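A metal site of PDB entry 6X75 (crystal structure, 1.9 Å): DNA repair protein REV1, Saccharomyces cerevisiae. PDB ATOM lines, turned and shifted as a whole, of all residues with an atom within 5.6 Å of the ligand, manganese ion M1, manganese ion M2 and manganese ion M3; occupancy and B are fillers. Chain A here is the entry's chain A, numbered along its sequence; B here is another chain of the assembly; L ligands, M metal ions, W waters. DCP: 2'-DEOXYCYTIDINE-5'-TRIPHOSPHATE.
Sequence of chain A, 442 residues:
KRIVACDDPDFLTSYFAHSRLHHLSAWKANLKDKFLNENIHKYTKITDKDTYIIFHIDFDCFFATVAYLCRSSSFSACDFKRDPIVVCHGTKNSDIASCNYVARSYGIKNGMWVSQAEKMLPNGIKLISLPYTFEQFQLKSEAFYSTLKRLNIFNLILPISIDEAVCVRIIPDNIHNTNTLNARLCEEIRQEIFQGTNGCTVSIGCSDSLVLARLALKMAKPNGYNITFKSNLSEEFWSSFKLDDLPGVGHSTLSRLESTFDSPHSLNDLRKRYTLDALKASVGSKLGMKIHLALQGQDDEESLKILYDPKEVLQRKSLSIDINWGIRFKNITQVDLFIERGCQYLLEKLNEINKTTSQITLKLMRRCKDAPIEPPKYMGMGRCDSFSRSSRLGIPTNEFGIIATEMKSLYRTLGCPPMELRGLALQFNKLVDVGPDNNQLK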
ATOM      1  N   ARG A  20      31.583 -19.240   4.811  1.00  0.00           N
ATOM      2  CA  ARG A  20      30.815 -20.348   4.283  1.00  0.00           C
ATOM      3  C   ARG A  20      31.046 -20.540   2.791  1.00  0.00           C
ATOM      4  O   ARG A  20      31.039 -21.681   2.313  1.00  0.00           O
ATOM      5  CB  ARG A  20      29.325 -20.193   4.596  1.00  0.00           C
ATOM      6  CG  ARG A  20      28.461 -19.680   3.454  1.00  0.00           C
ATOM      7  CD  ARG A  20      28.345 -18.162   3.453  1.00  0.00           C
ATOM      8  NE  ARG A  20      27.325 -17.760   2.485  1.00  0.00           N
ATOM      9  CZ  ARG A  20      27.082 -16.511   2.086  1.00  0.00           C
ATOM     10  NH1 ARG A  20      27.780 -15.499   2.570  1.00  0.00           N
ATOM     11  NH2 ARG A  20      26.118 -16.267   1.206  1.00  0.00           N
ATOM     12  N   LEU A  21      31.324 -19.447   2.050  1.00  0.00           N
ATOM     13  CA  LEU A  21      31.567 -19.636   0.615  1.00  0.00           C
ATOM     14  C   LEU A  21      32.906 -20.323   0.360  1.00  0.00           C
ATOM     15  O   LEU A  21      33.019 -21.124  -0.581  1.00  0.00           O
ATOM     16  CB  LEU A  21      31.487 -18.308  -0.141  1.00  0.00           C
ATOM     17  CG  LEU A  21      30.131 -17.575  -0.097  1.00  0.00           C
ATOM     18  CD1 LEU A  21      30.189 -16.164  -0.677  1.00  0.00           C
ATOM     19  CD2 LEU A  21      29.065 -18.374  -0.810  1.00  0.00           C
ATOM     20  N   LEU A  24      32.058 -23.997   0.909  1.00  0.00           N
ATOM     21  CA  LEU A  24      31.360 -24.566  -0.252  1.00  0.00           C
ATOM     22  C   LEU A  24      32.336 -24.930  -1.365  1.00  0.00           C
ATOM     23  O   LEU A  24      32.279 -26.025  -1.940  1.00  0.00           O
ATOM     24  CB  LEU A  24      30.307 -23.587  -0.788  1.00  0.00           C
ATOM     25  CG  LEU A  24      29.161 -23.262   0.167  1.00  0.00           C
ATOM     26  CD1 LEU A  24      28.274 -22.164  -0.399  1.00  0.00           C
ATOM     27  CD2 LEU A  24      28.346 -24.519   0.418  1.00  0.00           C
ATOM     28  N   ASP A  58      18.873 -33.033  -4.097  1.00  0.00           N
ATOM     29  CA  ASP A  58      19.382 -31.837  -3.411  1.00  0.00           C
ATOM     30  C   ASP A  58      18.704 -31.675  -2.047  1.00  0.00           C
ATOM     31  O   ASP A  58      17.476 -31.768  -1.958  1.00  0.00           O
ATOM     32  CB  ASP A  58      19.132 -30.610  -4.311  1.00  0.00           C
ATOM     33  CG  ASP A  58      19.688 -29.343  -3.720  1.00  0.00           C
ATOM     34  OD1 ASP A  58      19.024 -28.758  -2.833  1.00  0.00           O
ATOM     35  OD2 ASP A  58      20.767 -28.921  -4.177  1.00  0.00           O
ATOM     36  N   PHE A  59      19.495 -31.405  -1.008  1.00  0.00           N
ATOM     37  CA  PHE A  59      18.931 -31.159   0.328  1.00  0.00           C
ATOM     38  C   PHE A  59      18.025 -29.922   0.341  1.00  0.00           C
ATOM     39  O   PHE A  59      18.375 -28.886  -0.206  1.00  0.00           O
ATOM     40  CB  PHE A  59      20.036 -30.886   1.352  1.00  0.00           C
ATOM     41  CG  PHE A  59      20.776 -32.086   1.859  1.00  0.00           C
ATOM     42  CD1 PHE A  59      21.792 -32.665   1.119  1.00  0.00           C
ATOM     43  CD2 PHE A  59      20.531 -32.581   3.139  1.00  0.00           C
ATOM     44  CE1 PHE A  59      22.506 -33.732   1.599  1.00  0.00           C
ATOM     45  CE2 PHE A  59      21.255 -33.638   3.640  1.00  0.00           C
ATOM     46  CZ  PHE A  59      22.254 -34.221   2.876  1.00  0.00           C
ATOM     47  N   ASP A  60      16.900 -30.020   1.042  1.00  0.00           N
ATOM     48  CA  ASP A  60      16.088 -28.838   1.287  1.00  0.00           C
ATOM     49  C   ASP A  60      16.751 -27.964   2.338  1.00  0.00           C
ATOM     50  O   ASP A  60      17.249 -28.467   3.356  1.00  0.00           O
ATOM     51  CB  ASP A  60      14.678 -29.229   1.731  1.00  0.00           C
ATOM     52  CG  ASP A  60      14.059 -30.279   0.816  1.00  0.00           C
ATOM     53  OD1 ASP A  60      14.124 -30.087  -0.428  1.00  0.00           O
ATOM     54  OD2 ASP A  60      13.520 -31.274   1.324  1.00  0.00           O
ATOM     55  N   CYS A  61      16.739 -26.646   2.099  1.00  0.00           N
ATOM     56  CA  CYS A  61      17.451 -25.612   2.865  1.00  0.00           C
ATOM     57  C   CYS A  61      18.539 -26.205   3.750  1.00  0.00           C
ATOM     58  O   CYS A  61      18.419 -26.237   4.983  1.00  0.00           O
ATOM     59  CB  CYS A  61      16.462 -24.785   3.710  1.00  0.00           C
ATOM     60  SG  CYS A  61      15.249 -25.800   4.618  1.00  0.00           S
ATOM     61  N   PHE A  62      19.601 -26.672   3.097  1.00  0.00           N
ATOM     62  CA  PHE A  62      20.596 -27.559   3.715  1.00  0.00           C
ATOM     63  C   PHE A  62      21.164 -27.012   5.019  1.00  0.00           C
ATOM     64  O   PHE A  62      21.005 -27.624   6.080  1.00  0.00           O
ATOM     65  CB  PHE A  62      21.699 -27.785   2.698  1.00  0.00           C
ATOM     66  CG  PHE A  62      22.810 -28.676   3.189  1.00  0.00           C
ATOM     67  CD1 PHE A  62      22.544 -29.923   3.676  1.00  0.00           C
ATOM     68  CD2 PHE A  62      24.142 -28.261   3.105  1.00  0.00           C
ATOM     69  CE1 PHE A  62      23.549 -30.758   4.087  1.00  0.00           C
ATOM     70  CE2 PHE A  62      25.166 -29.074   3.511  1.00  0.00           C
ATOM     71  CZ  PHE A  62      24.876 -30.324   4.015  1.00  0.00           C
ATOM     72  N   PHE A  63      21.862 -25.855   4.959  1.00  0.00           N
ATOM     73  CA  PHE A  63      22.441 -25.295   6.183  1.00  0.00           C
ATOM     74  C   PHE A  63      21.369 -25.107   7.267  1.00  0.00           C
ATOM     75  O   PHE A  63      21.610 -25.406   8.440  1.00  0.00           O
ATOM     76  CB  PHE A  63      23.114 -23.954   5.909  1.00  0.00           C
ATOM     77  CG  PHE A  63      24.477 -24.042   5.241  1.00  0.00           C
ATOM     78  CD1 PHE A  63      24.944 -25.235   4.675  1.00  0.00           C
ATOM     79  CD2 PHE A  63      25.290 -22.915   5.175  1.00  0.00           C
ATOM     80  CE1 PHE A  63      26.197 -25.286   4.064  1.00  0.00           C
ATOM     81  CE2 PHE A  63      26.539 -22.949   4.568  1.00  0.00           C
ATOM     82  CZ  PHE A  63      26.989 -24.128   4.003  1.00  0.00           C
ATOM     83  N   ALA A  64      20.204 -24.593   6.882  1.00  0.00           N
ATOM     84  CA  ALA A  64      19.161 -24.329   7.887  1.00  0.00           C
ATOM     85  C   ALA A  64      18.712 -25.623   8.559  1.00  0.00           C
ATOM     86  O   ALA A  64      18.615 -25.702   9.784  1.00  0.00           O
ATOM     87  CB  ALA A  64      17.976 -23.619   7.242  1.00  0.00           C
ATOM     88  N   ILE A  96      22.365 -14.087   4.714  1.00  0.00           N
ATOM     89  CA  ILE A  96      21.615 -15.281   5.076  1.00  0.00           C
ATOM     90  C   ILE A  96      22.119 -16.394   4.166  1.00  0.00           C
ATOM     91  O   ILE A  96      21.909 -16.363   2.955  1.00  0.00           O
ATOM     92  CB  ILE A  96      20.098 -15.071   4.930  1.00  0.00           C
ATOM     93  CG1 ILE A  96      19.589 -14.203   6.082  1.00  0.00           C
ATOM     94  CG2 ILE A  96      19.367 -16.412   4.859  1.00  0.00           C
ATOM     95  CD1 ILE A  96      18.260 -13.556   5.758  1.00  0.00           C
ATOM     96  N   ALA A  97      22.847 -17.347   4.747  1.00  0.00           N
ATOM     97  CA  ALA A  97      23.388 -18.430   3.934  1.00  0.00           C
ATOM     98  C   ALA A  97      22.278 -19.360   3.484  1.00  0.00           C
ATOM     99  O   ALA A  97      22.246 -19.778   2.321  1.00  0.00           O
ATOM    100  CB  ALA A  97      24.457 -19.186   4.714  1.00  0.00           C
ATOM    101  N   SER A  98      21.367 -19.680   4.393  1.00  0.00           N
ATOM    102  CA  SER A  98      20.246 -20.558   4.085  1.00  0.00           C
ATOM    103  C   SER A  98      19.082 -20.142   4.967  1.00  0.00           C
ATOM    104  O   SER A  98      19.257 -19.690   6.106  1.00  0.00           O
ATOM    105  CB  SER A  98      20.630 -22.028   4.297  1.00  0.00           C
ATOM    106  OG  SER A  98      19.531 -22.894   4.068  1.00  0.00           O
ATOM    107  N   CYS A  99      17.890 -20.265   4.436  1.00  0.00           N
ATOM    108  CA  CYS A  99      16.698 -20.007   5.209  1.00  0.00           C
ATOM    109  C   CYS A  99      15.671 -21.084   4.938  1.00  0.00           C
ATOM    110  O   CYS A  99      15.617 -21.653   3.842  1.00  0.00           O
ATOM    111  CB  CYS A  99      16.167 -18.608   4.902  1.00  0.00           C
ATOM    112  SG  CYS A  99      15.628 -18.446   3.173  1.00  0.00           S
ATOM    113  N   TYR A 101      11.758 -22.908   4.862  1.00  0.00           N
ATOM    114  CA  TYR A 101      10.658 -22.581   3.972  1.00  0.00           C
ATOM    115  C   TYR A 101       9.608 -21.701   4.647  1.00  0.00           C
ATOM    116  O   TYR A 101       8.933 -20.948   3.950  1.00  0.00           O
ATOM    117  CB  TYR A 101      10.076 -23.889   3.403  1.00  0.00           C
ATOM    118  CG  TYR A 101      10.914 -24.301   2.210  1.00  0.00           C
ATOM    119  CD1 TYR A 101      12.173 -24.908   2.391  1.00  0.00           C
ATOM    120  CD2 TYR A 101      10.514 -24.006   0.902  1.00  0.00           C
ATOM    121  CE1 TYR A 101      12.976 -25.258   1.297  1.00  0.00           C
ATOM    122  CE2 TYR A 101      11.310 -24.351  -0.195  1.00  0.00           C
ATOM    123  CZ  TYR A 101      12.537 -24.965   0.014  1.00  0.00           C
ATOM    124  OH  TYR A 101      13.329 -25.315  -1.060  1.00  0.00           O
ATOM    125  N   ARG A 104      10.870 -18.420   3.770  1.00  0.00           N
ATOM    126  CA  ARG A 104      10.667 -18.110   2.360  1.00  0.00           C
ATOM    127  C   ARG A 104       9.219 -17.727   2.060  1.00  0.00           C
ATOM    128  O   ARG A 104       8.965 -16.997   1.085  1.00  0.00           O
ATOM    129  CB  ARG A 104      11.087 -19.300   1.506  1.00  0.00           C
ATOM    130  CG  ARG A 104      12.558 -19.692   1.725  1.00  0.00           C
ATOM    131  CD  ARG A 104      13.034 -20.778   0.776  1.00  0.00           C
ATOM    132  NE  ARG A 104      14.349 -21.262   1.195  1.00  0.00           N
ATOM    133  CZ  ARG A 104      15.162 -22.016   0.456  1.00  0.00           C
ATOM    134  NH1 ARG A 104      14.805 -22.378  -0.774  1.00  0.00           N
ATOM    135  NH2 ARG A 104      16.348 -22.389   0.966  1.00  0.00           N
ATOM    136  N   ASN A 110      17.904 -17.004   0.167  1.00  0.00           N
ATOM    137  CA  ASN A 110      19.324 -17.159   0.445  1.00  0.00           C
ATOM    138  C   ASN A 110      20.077 -15.976  -0.143  1.00  0.00           C
ATOM    139  O   ASN A 110      19.776 -15.523  -1.249  1.00  0.00           O
ATOM    140  CB  ASN A 110      19.868 -18.452  -0.173  1.00  0.00           C
ATOM    141  CG  ASN A 110      19.308 -19.696   0.498  1.00  0.00           C
ATOM    142  OD1 ASN A 110      18.658 -19.627   1.531  1.00  0.00           O
ATOM    143  ND2 ASN A 110      19.598 -20.855  -0.091  1.00  0.00           N
ATOM    144  N   GLY A 111      21.076 -15.484   0.590  1.00  0.00           N
ATOM    145  CA  GLY A 111      21.902 -14.404   0.104  1.00  0.00           C
ATOM    146  C   GLY A 111      21.419 -13.026   0.492  1.00  0.00           C
ATOM    147  O   GLY A 111      22.180 -12.059   0.335  1.00  0.00           O
ATOM    148  N   SER A 161      27.627 -30.418  -5.436  1.00  0.00           N
ATOM    149  CA  SER A 161      28.025 -29.590  -4.319  1.00  0.00           C
ATOM    150  C   SER A 161      27.988 -30.429  -3.060  1.00  0.00           C
ATOM    151  O   SER A 161      27.725 -31.648  -3.103  1.00  0.00           O
ATOM    152  CB  SER A 161      27.103 -28.369  -4.193  1.00  0.00           C
ATOM    153  OG  SER A 161      25.873 -28.712  -3.572  1.00  0.00           O
ATOM    154  N   ILE A 162      28.278 -29.773  -1.942  1.00  0.00           N
ATOM    155  CA  ILE A 162      28.086 -30.368  -0.619  1.00  0.00           C
ATOM    156  C   ILE A 162      26.692 -30.963  -0.455  1.00  0.00           C
ATOM    157  O   ILE A 162      26.519 -31.963   0.263  1.00  0.00           O
ATOM    158  CB  ILE A 162      28.384 -29.307   0.468  1.00  0.00           C
ATOM    159  CG1 ILE A 162      28.426 -29.963   1.848  1.00  0.00           C
ATOM    160  CG2 ILE A 162      27.331 -28.177   0.468  1.00  0.00           C
ATOM    161  CD1 ILE A 162      29.685 -30.821   2.075  1.00  0.00           C
ATOM    162  N   ASP A 163      25.655 -30.380  -1.069  1.00  0.00           N
ATOM    163  CA  ASP A 163      24.301 -30.824  -0.779  1.00  0.00           C
ATOM    164  C   ASP A 163      23.582 -31.364  -2.012  1.00  0.00           C
ATOM    165  O   ASP A 163      22.353 -31.427  -2.034  1.00  0.00           O
ATOM    166  CB  ASP A 163      23.487 -29.716  -0.095  1.00  0.00           C
ATOM    167  CG  ASP A 163      22.749 -28.817  -1.087  1.00  0.00           C
ATOM    168  OD1 ASP A 163      23.309 -28.425  -2.141  1.00  0.00           O
ATOM    169  OD2 ASP A 163      21.551 -28.531  -0.824  1.00  0.00           O
ATOM    170  N   GLU A 164      24.312 -31.772  -3.043  1.00  0.00           N
ATOM    171  CA  GLU A 164      23.631 -31.946  -4.316  1.00  0.00           C
ATOM    172  C   GLU A 164      24.413 -32.878  -5.211  1.00  0.00           C
ATOM    173  O   GLU A 164      25.630 -32.709  -5.356  1.00  0.00           O
ATOM    174  CB  GLU A 164      23.476 -30.575  -4.975  1.00  0.00           C
ATOM    175  CG  GLU A 164      22.812 -30.569  -6.317  1.00  0.00           C
ATOM    176  CD  GLU A 164      22.555 -29.149  -6.766  1.00  0.00           C
ATOM    177  OE1 GLU A 164      22.135 -28.962  -7.924  1.00  0.00           O
ATOM    178  OE2 GLU A 164      22.797 -28.217  -5.948  1.00  0.00           O
ATOM    179  N   ARG A 214      16.770 -30.639 -13.475  1.00  0.00           N
ATOM    180  CA  ARG A 214      16.995 -29.455 -12.643  1.00  0.00           C
ATOM    181  C   ARG A 214      15.700 -28.684 -12.433  1.00  0.00           C
ATOM    182  O   ARG A 214      15.394 -28.249 -11.312  1.00  0.00           O
ATOM    183  CB  ARG A 214      18.059 -28.560 -13.273  1.00  0.00           C
ATOM    184  CG  ARG A 214      18.323 -27.275 -12.483  1.00  0.00           C
ATOM    185  CD  ARG A 214      18.970 -27.578 -11.124  1.00  0.00           C
ATOM    186  NE  ARG A 214      19.074 -26.395 -10.265  1.00  0.00           N
ATOM    187  CZ  ARG A 214      18.137 -26.011  -9.405  1.00  0.00           C
ATOM    188  NH1 ARG A 214      17.012 -26.719  -9.296  1.00  0.00           N
ATOM    189  NH2 ARG A 214      18.314 -24.926  -8.665  1.00  0.00           N
ATOM    190  N   LYS A 221      10.474 -29.130  -4.851  1.00  0.00           N
ATOM    191  CA  LYS A 221      10.780 -28.613  -3.519  1.00  0.00           C
ATOM    192  C   LYS A 221       9.563 -27.923  -2.905  1.00  0.00           C
ATOM    193  O   LYS A 221       8.757 -27.326  -3.614  1.00  0.00           O
ATOM    194  CB  LYS A 221      11.946 -27.628  -3.587  1.00  0.00           C
ATOM    195  CG  LYS A 221      13.274 -28.308  -3.483  1.00  0.00           C
ATOM    196  CD  LYS A 221      14.428 -27.375  -3.776  1.00  0.00           C
ATOM    197  CE  LYS A 221      15.739 -28.156  -3.723  1.00  0.00           C
ATOM    198  NZ  LYS A 221      15.987 -28.722  -2.363  1.00  0.00           N
ATOM    199  P    DG B  12      23.481 -24.745 -10.530  1.00  0.00           P
ATOM    200  OP1  DG B  12      22.442 -25.791 -10.761  1.00  0.00           O
ATOM    201  OP2  DG B  12      23.072 -23.411 -10.063  1.00  0.00           O
ATOM    202  O5'  DG B  12      24.520 -25.387  -9.516  1.00  0.00           O
ATOM    203  C5'  DG B  12      24.857 -24.698  -8.367  1.00  0.00           C
ATOM    204  C4'  DG B  12      26.065 -25.323  -7.729  1.00  0.00           C
ATOM    205  O4'  DG B  12      27.234 -24.995  -8.535  1.00  0.00           O
ATOM    206  C3'  DG B  12      26.371 -24.768  -6.345  1.00  0.00           C
ATOM    207  O3'  DG B  12      25.745 -25.546  -5.328  1.00  0.00           O
ATOM    208  C2'  DG B  12      27.896 -24.889  -6.300  1.00  0.00           C
ATOM    209  C1'  DG B  12      28.235 -24.432  -7.708  1.00  0.00           C
ATOM    210  N9   DG B  12      28.200 -22.968  -7.835  1.00  0.00           N
ATOM    211  C8   DG B  12      27.256 -22.179  -8.478  1.00  0.00           C
ATOM    212  N7   DG B  12      27.497 -20.901  -8.365  1.00  0.00           N
ATOM    213  C5   DG B  12      28.661 -20.837  -7.607  1.00  0.00           C
ATOM    214  C6   DG B  12      29.424 -19.715  -7.152  1.00  0.00           C
ATOM    215  O6   DG B  12      29.210 -18.497  -7.343  1.00  0.00           O
ATOM    216  N1   DG B  12      30.533 -20.118  -6.405  1.00  0.00           N
ATOM    217  C2   DG B  12      30.874 -21.436  -6.133  1.00  0.00           C
ATOM    218  N2   DG B  12      31.980 -21.634  -5.415  1.00  0.00           N
ATOM    219  N3   DG B  12      30.183 -22.466  -6.553  1.00  0.00           N
ATOM    220  C4   DG B  12      29.098 -22.101  -7.267  1.00  0.00           C
ATOM    221  P    DC B  13      24.327 -25.106  -4.693  1.00  0.00           P
ATOM    222  OP1  DC B  13      23.998 -26.040  -3.586  1.00  0.00           O
ATOM    223  OP2  DC B  13      23.384 -24.985  -5.827  1.00  0.00           O
ATOM    224  O5'  DC B  13      24.538 -23.638  -4.111  1.00  0.00           O
ATOM    225  C5'  DC B  13      25.641 -23.338  -3.276  1.00  0.00           C
ATOM    226  C4'  DC B  13      26.387 -22.107  -3.786  1.00  0.00           C
ATOM    227  O4'  DC B  13      26.071 -21.873  -5.182  1.00  0.00           O
ATOM    228  C3'  DC B  13      26.077 -20.800  -3.063  1.00  0.00           C
ATOM    229  O3'  DC B  13      27.291 -20.127  -2.751  1.00  0.00           O
ATOM    230  C2'  DC B  13      25.257 -20.012  -4.097  1.00  0.00           C
ATOM    231  C1'  DC B  13      25.902 -20.495  -5.372  1.00  0.00           C
ATOM    232  N1   DC B  13      25.092 -20.267  -6.595  1.00  0.00           N
ATOM    233  C2   DC B  13      25.057 -18.990  -7.177  1.00  0.00           C
ATOM    234  O2   DC B  13      25.671 -18.055  -6.637  1.00  0.00           O
ATOM    235  N3   DC B  13      24.336 -18.803  -8.318  1.00  0.00           N
ATOM    236  C4   DC B  13      23.689 -19.831  -8.872  1.00  0.00           C
ATOM    237  N4   DC B  13      22.984 -19.599  -9.984  1.00  0.00           N
ATOM    238  C5   DC B  13      23.718 -21.144  -8.300  1.00  0.00           C
ATOM    239  C6   DC B  13      24.432 -21.317  -7.177  1.00  0.00           C
HETATM  240  N1  DCP L   1      24.356 -21.173   0.270  1.00  0.00           N
HETATM  241  C2  DCP L   1      25.028 -19.928   0.709  1.00  0.00           C
HETATM  242  N3  DCP L   1      24.723 -18.646   0.040  1.00  0.00           N
HETATM  243  C4  DCP L   1      23.768 -18.606  -1.031  1.00  0.00           C
HETATM  244  C5  DCP L   1      23.078 -19.865  -1.480  1.00  0.00           C
HETATM  245  C6  DCP L   1      23.399 -21.148  -0.817  1.00  0.00           C
HETATM  246  O2  DCP L   1      25.799 -19.999   1.606  1.00  0.00           O
HETATM  247  N4  DCP L   1      23.498 -17.347  -1.672  1.00  0.00           N
HETATM  248  C1' DCP L   1      24.721 -22.359   1.004  1.00  0.00           C
HETATM  249  C2' DCP L   1      23.799 -22.570   1.953  1.00  0.00           C
HETATM  250  C3' DCP L   1      22.801 -23.671   1.313  1.00  0.00           C
HETATM  251  C4' DCP L   1      23.689 -24.535   0.713  1.00  0.00           C
HETATM  252  O4' DCP L   1      24.672 -23.594   0.045  1.00  0.00           O
HETATM  253  O3' DCP L   1      22.032 -24.273   2.358  1.00  0.00           O
HETATM  254  C5' DCP L   1      23.107 -25.301  -0.451  1.00  0.00           C
HETATM  255  O5' DCP L   1      22.743 -24.352  -1.430  1.00  0.00           O
HETATM  256  PA  DCP L   1      21.312 -24.590  -2.191  1.00  0.00           P
HETATM  257  O1A DCP L   1      21.113 -26.092  -2.458  1.00  0.00           O
HETATM  258  O2A DCP L   1      21.257 -23.757  -3.459  1.00  0.00           O
HETATM  259  O3A DCP L   1      20.087 -23.961  -1.212  1.00  0.00           O
HETATM  260  PB  DCP L   1      19.398 -24.609   0.103  1.00  0.00           P
HETATM  261  O1B DCP L   1      19.620 -23.729   1.345  1.00  0.00           O
HETATM  262  O2B DCP L   1      19.849 -26.079   0.264  1.00  0.00           O
HETATM  263  O3B DCP L   1      17.754 -24.529  -0.154  1.00  0.00           O
HETATM  264  PG  DCP L   1      16.961 -25.320  -1.380  1.00  0.00           P
HETATM  265  O1G DCP L   1      15.918 -26.249  -0.708  1.00  0.00           O
HETATM  266  O2G DCP L   1      16.299 -24.262  -2.253  1.00  0.00           O
HETATM  267  O3G DCP L   1      17.945 -26.121  -2.180  1.00  0.00           O
HETATM  268 MN    MN M   1      19.653 -27.437  -1.342  1.00  0.00          MN
HETATM  269 MN    MN M   2      21.285 -23.640  -5.444  1.00  0.00          MN
HETATM  270 MN    MN M   3      22.170 -27.317  -3.866  1.00  0.00          MN
HETATM  271  O   HOH W   1      21.153 -26.100  -5.473  1.00  0.00           O
HETATM  272  O   HOH W   2      18.781 -23.408  -5.579  1.00  0.00           O
HETATM  273  O   HOH W   3      21.919 -17.309  -4.094  1.00  0.00           O
HETATM  274  O   HOH W   4      21.318 -23.542  -8.050  1.00  0.00           O
HETATM  275  O   HOH W   5      18.522 -25.901  -4.773  1.00  0.00           O
HETATM  276  O   HOH W   6      25.423 -15.073  -1.431  1.00  0.00           O
HETATM  277  O   HOH W   7      20.148 -20.911  -2.799  1.00  0.00           O
HETATM  278  O   HOH W   8      21.664 -21.235  -4.971  1.00  0.00           O
HETATM  279  O   HOH W   9      17.507 -21.971  -3.138  1.00  0.00           O
HETATM  280  O   HOH W  10      15.206 -24.070  -4.611  1.00  0.00           O
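O of Asp 58 lies within hydrogen-bond range of NZ of Lys 221, 3.4 Å away. The side-chain amino group (NZ) of Lys 221 sits close to the backbone carbonyl oxygen (O) of Phe 59. OP1 of DC 13 of chain B sits close to the side-chain hydroxyl of Ser 161 (3.3 Å). The backbone NH (N) of Asp 163 sits at hydrogen-bond distance from the side-chain hydroxyl (OG) of Ser 161 (3.0 Å). NE of Arg 104 is in hydrogen-bond range of O of Cys 99 (3.0 Å). The side-chain hydroxyl of Ser 98 lies within hydrogen-bond range of the backbone NH of Ala 64 (3.4 Å). The side-chain amide oxygen (OD1) of Asn 110 lies within hydrogen-bond range of the backbone NH (N) of Cys 99 (3.1 Å). O of Ile 96 lies within hydrogen-bond range of N of Gly 111, at 2.7 Å.
The side-chain carboxylate (OD1) of Asp 58 is bound to manganese ion M1. Manganese ion M1 is bound by O2B of the ligand (2.1 Å). Manganese ion M1 is bound by the backbone carbonyl oxygen (O) of Phe 59 (2.2 Å). The side-chain carboxylate (OD2) of Asp 163 is bound to manganese ion M1 (2.3 Å). An oxygen (O1A) of the ligand binds manganese ion M1 (2.3 Å). Manganese ion M1 is bound by an oxygen (O3G) of the ligand.
Manganese ion M3 is bound by O1A of the ligand (2.1 Å), OD2 of Asp 58 (2.2 Å), OP1 of DC 13 of chain B (2.2 Å), water W1 (2.3 Å), OD1 of Asp 163 (2.3 Å) and OE2 of Glu 164 (2.4 Å). Manganese ion M3 has six donor atoms within binding distance.
The side-chain hydroxyl (OH) of Tyr 101 sits at hydrogen-bond distance from an oxygen (O1G) of the ligand (2.8 Å). The guanidinium group (NH1) of Arg 104 lies within salt-bridge range of an oxygen (O2G) of the ligand (2.8 Å). NE of Arg 20 lies within hydrogen-bond range of O2 of the ligand, at 2.8 Å. O1B of the ligand lies within hydrogen-bond range of OG of Ser 98, at 2.8 Å. An oxygen (O1B) of the ligand sits at hydrogen-bond distance from the backbone NH (N) of Phe 62. The backbone NH (N) of Cys 61 is in hydrogen-bond range of an oxygen (O1G) of the ligand. The side-chain amino group (NZ) of Lys 221 lies within salt-bridge range of an oxygen (O1G) of the ligand (3.0 Å). An oxygen (O3') of the ligand sits at hydrogen-bond distance from the backbone NH of Phe 63 (3.0 Å). The side-chain amide nitrogen (ND2) of Asn 110 lies within hydrogen-bond range of an oxygen (O1B) of the ligand.
Of the 26 residues printed, 3 come within 4 Å of manganese ion M1. The nearest printed residue that does not touch manganese ion M1 is Lys 221 (4.02 Å).
Manganese ion M2 is bound by an oxygen (O2A) of the ligand, water W1, water W8, water W2, OP2 of DC 13 of chain B and water W4. Manganese ion M2 has six donor atoms within binding distance.
Water W4 bridges OP2 of DG 12 of chain B (2.7 Å) and NH2 of Arg 214 (3.4 Å). Water W6 lies within hydrogen-bond range of the guanidinium group of Arg 20 and a nitrogen (N4) of the ligand. Water W7 lies within hydrogen-bond range of the side-chain amide nitrogen (ND2) of Asn 110 (2.8 Å) and an oxygen (O3A) of the ligand (3.4 Å).
Ser 161 touches manganese ion M3. The nearest printed residue that does not touch manganese ion M3 is DG 12 of chain B (4.2 Å).
One residue has an atom within 4 Å of manganese ion M2: DC 13 of chain B.
The backbone carbonyl oxygen (O) of Ala 97 lies close to a nitrogen (N1) of the ligand (3.3 Å). Residues that only touch the ligand: Asp 60, Gly 111 and Leu 24. Hydrophobic or aromatic side chains that line the ligand: Leu 24, Phe 62, Phe 63, Ala 97 and Tyr 101. Of the 26 residues printed, 17 come within 4 Å of the ligand.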
